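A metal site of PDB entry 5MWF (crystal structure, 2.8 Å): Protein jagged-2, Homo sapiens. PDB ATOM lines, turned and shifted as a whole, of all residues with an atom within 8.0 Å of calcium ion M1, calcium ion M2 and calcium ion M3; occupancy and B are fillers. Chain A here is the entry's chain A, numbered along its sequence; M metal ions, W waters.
Calcium ion M3 is bound by OD1 of Asp 126, 2.2 Å away.
Calcium ion M3 is bound by O of Trp 125, 2.4 Å away.
OD2 of Asp 25 is bound to calcium ion M3 (2.5 Å).
The side-chain carboxylate (OD1) of Asp 25 binds calcium ion M3 (2.5 Å).
Calcium ion M3 is bound by OD1 of Asp 124 (2.5 Å).
Calcium ion M3 is bound by the side-chain carboxylate (OD2) of Asp 42, 2.5 Å away.
Slightly farther from calcium ion M3 lies the side-chain carboxylate (OD2) of Asp 124 (3.0 Å).
Five residues have an atom within 4 Å of calcium ion M3: Asp 25, Asp 42, Asp 124, Trp 125 and Asp 126.
The nearest printed residue that does not touch calcium ion M3 is Glu 40 (4.8 Å).
Within 4 Å of calcium ion M2: Asp 25, Asp 39, Glu 40 and Asp 42.
The nearest printed residue that does not touch calcium ion M2 is Cys 41 (4.4 Å).
CD2 of Leu 135 touches calcium ion M1, at 3.9 Å.
Within 4 Å of calcium ion M1: Cys 24, Asp 25, Asp 124, Asp 126 and Leu 135.
The nearest printed residue that does not touch calcium ion M1 is Trp 125 (5.1 Å).
Calcium ion M1 is bound by OD1 of Asp 25, at 2.4 Å.
The side-chain carboxylate (OD2) of Asp 126 binds calcium ion M1 (2.4 Å).
Calcium ion M1 is bound by OD1 of Asp 126 (2.5 Å).
OD2 of Asp 124 is bound to calcium ion M1 (2.5 Å).
Calcium ion M1 is bound by O of Cys 24 (2.7 Å).
Calcium ion M1 has five donor atoms within binding distance.
ND2 of Asn 127 sits close to NE1 of Trp 125, at 3.4 Å.
O of Leu 135 is in hydrogen-bond range of N of Asp 124.
The side-chain sulfur (SG) of Cys 24 is disulfide-bonded to the side-chain sulfur (SG) of Cys 41, 2.0 Å away.
Calcium ion M2 is bound by the side-chain carboxylate (OD1) of Asp 39, the side-chain carboxylate (OD2) of Asp 25, the backbone carbonyl oxygen (O) of Glu 40, the side-chain carboxylate (OD1) of Asp 42 and the side-chain carboxylate (OD2) of Asp 42.
Calcium ion M2 has five donor atoms within binding distance.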
ATOM      1  N   LEU A  18       6.453  -1.798  31.079  1.00  0.00           N
ATOM      2  CA  LEU A  18       7.055  -1.253  29.878  1.00  0.00           C
ATOM      3  C   LEU A  18       6.863   0.250  29.904  1.00  0.00           C
ATOM      4  O   LEU A  18       6.184   0.793  30.772  1.00  0.00           O
ATOM      5  CB  LEU A  18       6.440  -1.871  28.614  1.00  0.00           C
ATOM      6  CG  LEU A  18       6.458  -3.400  28.512  1.00  0.00           C
ATOM      7  CD1 LEU A  18       5.398  -3.887  27.538  1.00  0.00           C
ATOM      8  CD2 LEU A  18       7.822  -3.903  28.111  1.00  0.00           C
ATOM      9  N   CYS A  23       2.289  -4.507  31.678  1.00  0.00           N
ATOM     10  CA  CYS A  23       3.286  -5.422  32.187  1.00  0.00           C
ATOM     11  C   CYS A  23       4.020  -6.074  31.029  1.00  0.00           C
ATOM     12  O   CYS A  23       3.491  -6.221  29.926  1.00  0.00           O
ATOM     13  CB  CYS A  23       2.634  -6.492  33.081  1.00  0.00           C
ATOM     14  SG  CYS A  23       1.736  -5.886  34.541  1.00  0.00           S
ATOM     15  N   CYS A  24       5.272  -6.471  31.291  1.00  0.00           N
ATOM     16  CA  CYS A  24       6.131  -6.991  30.230  1.00  0.00           C
ATOM     17  C   CYS A  24       5.524  -8.238  29.588  1.00  0.00           C
ATOM     18  O   CYS A  24       5.324  -8.285  28.364  1.00  0.00           O
ATOM     19  CB  CYS A  24       7.524  -7.303  30.784  1.00  0.00           C
ATOM     20  SG  CYS A  24       8.606  -5.886  31.001  1.00  0.00           S
ATOM     21  N   ASP A  25       5.224  -9.243  30.405  1.00  0.00           N
ATOM     22  CA  ASP A  25       4.697 -10.514  29.918  1.00  0.00           C
ATOM     23  C   ASP A  25       3.383 -10.784  30.640  1.00  0.00           C
ATOM     24  O   ASP A  25       3.377 -11.124  31.821  1.00  0.00           O
ATOM     25  CB  ASP A  25       5.697 -11.650  30.141  1.00  0.00           C
ATOM     26  CG  ASP A  25       6.918 -11.530  29.258  1.00  0.00           C
ATOM     27  OD1 ASP A  25       6.840 -10.864  28.209  1.00  0.00           O
ATOM     28  OD2 ASP A  25       7.969 -12.117  29.609  1.00  0.00           O
ATOM     29  N   GLY A  26       2.280 -10.615  29.923  1.00  0.00           N
ATOM     30  CA  GLY A  26       0.983 -10.869  30.494  1.00  0.00           C
ATOM     31  C   GLY A  26      -0.019  -9.766  30.246  1.00  0.00           C
ATOM     32  O   GLY A  26       0.292  -8.582  30.393  1.00  0.00           O
ATOM     33  N   HIS A  38       4.666 -13.213  38.224  1.00  0.00           N
ATOM     34  CA  HIS A  38       5.948 -13.901  38.318  1.00  0.00           C
ATOM     35  C   HIS A  38       6.653 -14.051  36.982  1.00  0.00           C
ATOM     36  O   HIS A  38       7.857 -14.298  36.970  1.00  0.00           O
ATOM     37  CB  HIS A  38       5.775 -15.298  38.923  1.00  0.00           C
ATOM     38  CG  HIS A  38       5.433 -15.300  40.385  1.00  0.00           C
ATOM     39  ND1 HIS A  38       5.430 -16.453  41.139  1.00  0.00           N
ATOM     40  CD2 HIS A  38       5.091 -14.302  41.221  1.00  0.00           C
ATOM     41  CE1 HIS A  38       5.104 -16.156  42.391  1.00  0.00           C
ATOM     42  NE2 HIS A  38       4.889 -14.856  42.457  1.00  0.00           N
ATOM     43  N   ASP A  39       5.943 -13.889  35.867  1.00  0.00           N
ATOM     44  CA  ASP A  39       6.618 -13.809  34.569  1.00  0.00           C
ATOM     45  C   ASP A  39       7.181 -12.396  34.445  1.00  0.00           C
ATOM     46  O   ASP A  39       6.459 -11.454  34.128  1.00  0.00           O
ATOM     47  CB  ASP A  39       5.662 -14.146  33.435  1.00  0.00           C
ATOM     48  CG  ASP A  39       6.393 -14.484  32.150  1.00  0.00           C
ATOM     49  OD1 ASP A  39       7.548 -14.041  31.988  1.00  0.00           O
ATOM     50  OD2 ASP A  39       5.808 -15.188  31.297  1.00  0.00           O
ATOM     51  N   GLU A  40       8.480 -12.257  34.694  1.00  0.00           N
ATOM     52  CA  GLU A  40       9.141 -10.974  34.726  1.00  0.00           C
ATOM     53  C   GLU A  40       9.585 -10.540  33.321  1.00  0.00           C
ATOM     54  O   GLU A  40       9.449 -11.280  32.347  1.00  0.00           O
ATOM     55  CB  GLU A  40      10.355 -11.005  35.668  1.00  0.00           C
ATOM     56  CG  GLU A  40      10.027 -11.404  37.094  1.00  0.00           C
ATOM     57  CD  GLU A  40      11.240 -11.364  38.002  1.00  0.00           C
ATOM     58  OE1 GLU A  40      11.115 -10.878  39.150  1.00  0.00           O
ATOM     59  OE2 GLU A  40      12.328 -11.815  37.579  1.00  0.00           O
ATOM     60  N   CYS A  41      10.090  -9.318  33.245  1.00  0.00           N
ATOM     61  CA  CYS A  41      10.671  -8.818  31.999  1.00  0.00           C
ATOM     62  C   CYS A  41      11.914  -9.617  31.657  1.00  0.00           C
ATOM     63  O   CYS A  41      12.728  -9.945  32.527  1.00  0.00           O
ATOM     64  CB  CYS A  41      11.012  -7.341  32.113  1.00  0.00           C
ATOM     65  SG  CYS A  41       9.657  -6.313  32.688  1.00  0.00           S
ATOM     66  N   ASP A  42      12.054  -9.961  30.382  1.00  0.00           N
ATOM     67  CA  ASP A  42      13.237 -10.658  29.863  1.00  0.00           C
ATOM     68  C   ASP A  42      14.123  -9.590  29.216  1.00  0.00           C
ATOM     69  O   ASP A  42      14.059  -9.339  28.011  1.00  0.00           O
ATOM     70  CB  ASP A  42      12.802 -11.741  28.880  1.00  0.00           C
ATOM     71  CG  ASP A  42      11.732 -12.651  29.471  1.00  0.00           C
ATOM     72  OD1 ASP A  42      11.854 -12.997  30.675  1.00  0.00           O
ATOM     73  OD2 ASP A  42      10.739 -12.980  28.779  1.00  0.00           O
ATOM     74  N   THR A  43      14.969  -8.970  30.031  1.00  0.00           N
ATOM     75  CA  THR A  43      15.575  -7.686  29.696  1.00  0.00           C
ATOM     76  C   THR A  43      16.896  -7.851  28.962  1.00  0.00           C
ATOM     77  O   THR A  43      17.790  -8.555  29.435  1.00  0.00           O
ATOM     78  CB  THR A  43      15.797  -6.856  30.958  1.00  0.00           C
ATOM     79  OG1 THR A  43      14.554  -6.680  31.652  1.00  0.00           O
ATOM     80  CG2 THR A  43      16.357  -5.484  30.603  1.00  0.00           C
ATOM     81  N   VAL A  71      19.583 -11.640  26.813  1.00  0.00           N
ATOM     82  CA  VAL A  71      18.825 -11.374  28.020  1.00  0.00           C
ATOM     83  C   VAL A  71      19.757 -11.452  29.219  1.00  0.00           C
ATOM     84  O   VAL A  71      20.388 -12.492  29.469  1.00  0.00           O
ATOM     85  CB  VAL A  71      17.655 -12.362  28.167  1.00  0.00           C
ATOM     86  CG1 VAL A  71      16.983 -12.179  29.520  1.00  0.00           C
ATOM     87  CG2 VAL A  71      16.649 -12.144  27.051  1.00  0.00           C
ATOM     88  N   GLY A  73      18.777 -10.508  32.529  1.00  0.00           N
ATOM     89  CA  GLY A  73      18.111 -10.856  33.764  1.00  0.00           C
ATOM     90  C   GLY A  73      16.620 -10.564  33.713  1.00  0.00           C
ATOM     91  O   GLY A  73      16.016 -10.508  32.638  1.00  0.00           O
ATOM     92  N   GLY A  74      16.041 -10.382  34.892  1.00  0.00           N
ATOM     93  CA  GLY A  74      14.619 -10.145  35.013  1.00  0.00           C
ATOM     94  C   GLY A  74      14.258  -8.683  35.134  1.00  0.00           C
ATOM     95  O   GLY A  74      14.767  -7.849  34.395  1.00  0.00           O
ATOM     96  N   ASN A  75      13.385  -8.359  36.092  1.00  0.00           N
ATOM     97  CA  ASN A  75      12.966  -6.976  36.273  1.00  0.00           C
ATOM     98  C   ASN A  75      14.101  -6.116  36.813  1.00  0.00           C
ATOM     99  O   ASN A  75      14.248  -4.954  36.408  1.00  0.00           O
ATOM    100  CB  ASN A  75      11.766  -6.902  37.202  1.00  0.00           C
ATOM    101  CG  ASN A  75      10.559  -7.620  36.651  1.00  0.00           C
ATOM    102  OD1 ASN A  75      10.430  -7.808  35.437  1.00  0.00           O
ATOM    103  ND2 ASN A  75       9.662  -8.038  37.540  1.00  0.00           N
ATOM    104  N   TRP A 123      14.889  -3.542  26.450  1.00  0.00           N
ATOM    105  CA  TRP A 123      13.809  -4.193  25.733  1.00  0.00           C
ATOM    106  C   TRP A 123      13.419  -5.507  26.402  1.00  0.00           C
ATOM    107  O   TRP A 123      14.252  -6.181  27.011  1.00  0.00           O
ATOM    108  CB  TRP A 123      14.201  -4.479  24.272  1.00  0.00           C
ATOM    109  CG  TRP A 123      14.378  -3.269  23.406  1.00  0.00           C
ATOM    110  CD1 TRP A 123      15.496  -2.493  23.302  1.00  0.00           C
ATOM    111  CD2 TRP A 123      13.412  -2.698  22.528  1.00  0.00           C
ATOM    112  NE1 TRP A 123      15.286  -1.471  22.397  1.00  0.00           N
ATOM    113  CE2 TRP A 123      14.007  -1.586  21.911  1.00  0.00           C
ATOM    114  CE3 TRP A 123      12.089  -3.027  22.197  1.00  0.00           C
ATOM    115  CZ2 TRP A 123      13.328  -0.788  20.987  1.00  0.00           C
ATOM    116  CZ3 TRP A 123      11.424  -2.241  21.274  1.00  0.00           C
ATOM    117  CH2 TRP A 123      12.043  -1.135  20.685  1.00  0.00           C
ATOM    118  N   ASP A 124      12.135  -5.854  26.270  1.00  0.00           N
ATOM    119  CA  ASP A 124      11.633  -7.162  26.674  1.00  0.00           C
ATOM    120  C   ASP A 124      11.715  -8.127  25.504  1.00  0.00           C
ATOM    121  O   ASP A 124      11.418  -7.775  24.356  1.00  0.00           O
ATOM    122  CB  ASP A 124      10.180  -7.061  27.170  1.00  0.00           C
ATOM    123  CG  ASP A 124       9.573  -8.418  27.511  1.00  0.00           C
ATOM    124  OD1 ASP A 124      10.293  -9.310  28.001  1.00  0.00           O
ATOM    125  OD2 ASP A 124       8.351  -8.600  27.284  1.00  0.00           O
ATOM    126  N   TRP A 125      12.123  -9.359  25.809  1.00  0.00           N
ATOM    127  CA  TRP A 125      12.352 -10.401  24.811  1.00  0.00           C
ATOM    128  C   TRP A 125      11.229 -11.424  24.887  1.00  0.00           C
ATOM    129  O   TRP A 125      10.921 -11.931  25.981  1.00  0.00           O
ATOM    130  CB  TRP A 125      13.715 -11.057  25.027  1.00  0.00           C
ATOM    131  CG  TRP A 125      14.063 -12.144  24.064  1.00  0.00           C
ATOM    132  CD1 TRP A 125      14.203 -13.470  24.330  1.00  0.00           C
ATOM    133  CD2 TRP A 125      14.318 -12.000  22.663  1.00  0.00           C
ATOM    134  NE1 TRP A 125      14.524 -14.164  23.205  1.00  0.00           N
ATOM    135  CE2 TRP A 125      14.605 -13.284  22.152  1.00  0.00           C
ATOM    136  CE3 TRP A 125      14.329 -10.906  21.779  1.00  0.00           C
ATOM    137  CZ2 TRP A 125      14.895 -13.509  20.811  1.00  0.00           C
ATOM    138  CZ3 TRP A 125      14.621 -11.137  20.445  1.00  0.00           C
ATOM    139  CH2 TRP A 125      14.899 -12.421  19.977  1.00  0.00           C
ATOM    140  N   ASP A 126      10.625 -11.721  23.737  1.00  0.00           N
ATOM    141  CA  ASP A 126       9.595 -12.746  23.639  1.00  0.00           C
ATOM    142  C   ASP A 126       9.929 -13.772  22.558  1.00  0.00           C
ATOM    143  O   ASP A 126       9.026 -14.301  21.901  1.00  0.00           O
ATOM    144  CB  ASP A 126       8.209 -12.129  23.385  1.00  0.00           C
ATOM    145  CG  ASP A 126       7.840 -11.066  24.401  1.00  0.00           C
ATOM    146  OD1 ASP A 126       8.197 -11.213  25.593  1.00  0.00           O
ATOM    147  OD2 ASP A 126       7.146 -10.091  24.024  1.00  0.00           O
ATOM    148  N   ASN A 127      11.217 -14.066  22.376  1.00  0.00           N
ATOM    149  CA  ASN A 127      11.677 -15.096  21.453  1.00  0.00           C
ATOM    150  C   ASN A 127      11.113 -14.891  20.051  1.00  0.00           C
ATOM    151  O   ASN A 127      10.659 -15.831  19.391  1.00  0.00           O
ATOM    152  CB  ASN A 127      11.353 -16.490  21.985  1.00  0.00           C
ATOM    153  CG  ASN A 127      12.120 -16.816  23.255  1.00  0.00           C
ATOM    154  OD1 ASN A 127      11.637 -16.554  24.352  1.00  0.00           O
ATOM    155  ND2 ASN A 127      13.317 -17.371  23.099  1.00  0.00           N
ATOM    156  N   ASN A 132       9.050  -4.768  17.312  1.00  0.00           N
ATOM    157  CA  ASN A 132       7.796  -4.448  17.994  1.00  0.00           C
ATOM    158  C   ASN A 132       8.077  -3.333  18.994  1.00  0.00           C
ATOM    159  O   ASN A 132       8.556  -3.599  20.107  1.00  0.00           O
ATOM    160  CB  ASN A 132       7.217  -5.676  18.671  1.00  0.00           C
ATOM    161  CG  ASN A 132       5.814  -5.445  19.232  1.00  0.00           C
ATOM    162  OD1 ASN A 132       5.365  -4.302  19.357  1.00  0.00           O
ATOM    163  ND2 ASN A 132       5.141  -6.524  19.594  1.00  0.00           N
ATOM    164  N   GLU A 134       6.393  -1.741  20.961  1.00  0.00           N
ATOM    165  CA  GLU A 134       5.649  -1.771  22.215  1.00  0.00           C
ATOM    166  C   GLU A 134       6.333  -2.592  23.289  1.00  0.00           C
ATOM    167  O   GLU A 134       5.815  -2.678  24.404  1.00  0.00           O
ATOM    168  CB  GLU A 134       4.230  -2.299  21.962  1.00  0.00           C
ATOM    169  CG  GLU A 134       3.487  -1.484  20.926  1.00  0.00           C
ATOM    170  CD  GLU A 134       2.017  -1.374  21.209  1.00  0.00           C
ATOM    171  OE1 GLU A 134       1.218  -1.864  20.381  1.00  0.00           O
ATOM    172  OE2 GLU A 134       1.665  -0.804  22.267  1.00  0.00           O
ATOM    173  N   LEU A 135       7.476  -3.211  22.978  1.00  0.00           N
ATOM    174  CA  LEU A 135       8.257  -3.953  23.957  1.00  0.00           C
ATOM    175  C   LEU A 135       9.375  -3.122  24.572  1.00  0.00           C
ATOM    176  O   LEU A 135      10.279  -3.679  25.202  1.00  0.00           O
ATOM    177  CB  LEU A 135       8.824  -5.225  23.321  1.00  0.00           C
ATOM    178  CG  LEU A 135       7.819  -6.115  22.571  1.00  0.00           C
ATOM    179  CD1 LEU A 135       8.561  -7.105  21.690  1.00  0.00           C
ATOM    180  CD2 LEU A 135       6.907  -6.833  23.551  1.00  0.00           C
HETATM  181 CA    CA M   1       6.346  -9.666  26.235  1.00  0.00          CA
HETATM  182 CA    CA M   2       9.484 -13.230  30.995  1.00  0.00          CA
HETATM  183 CA    CA M   3       9.138 -11.489  27.540  1.00  0.00          CA
HETATM  184  O   HOH W   1       3.154 -10.599  26.250  1.00  0.00           O
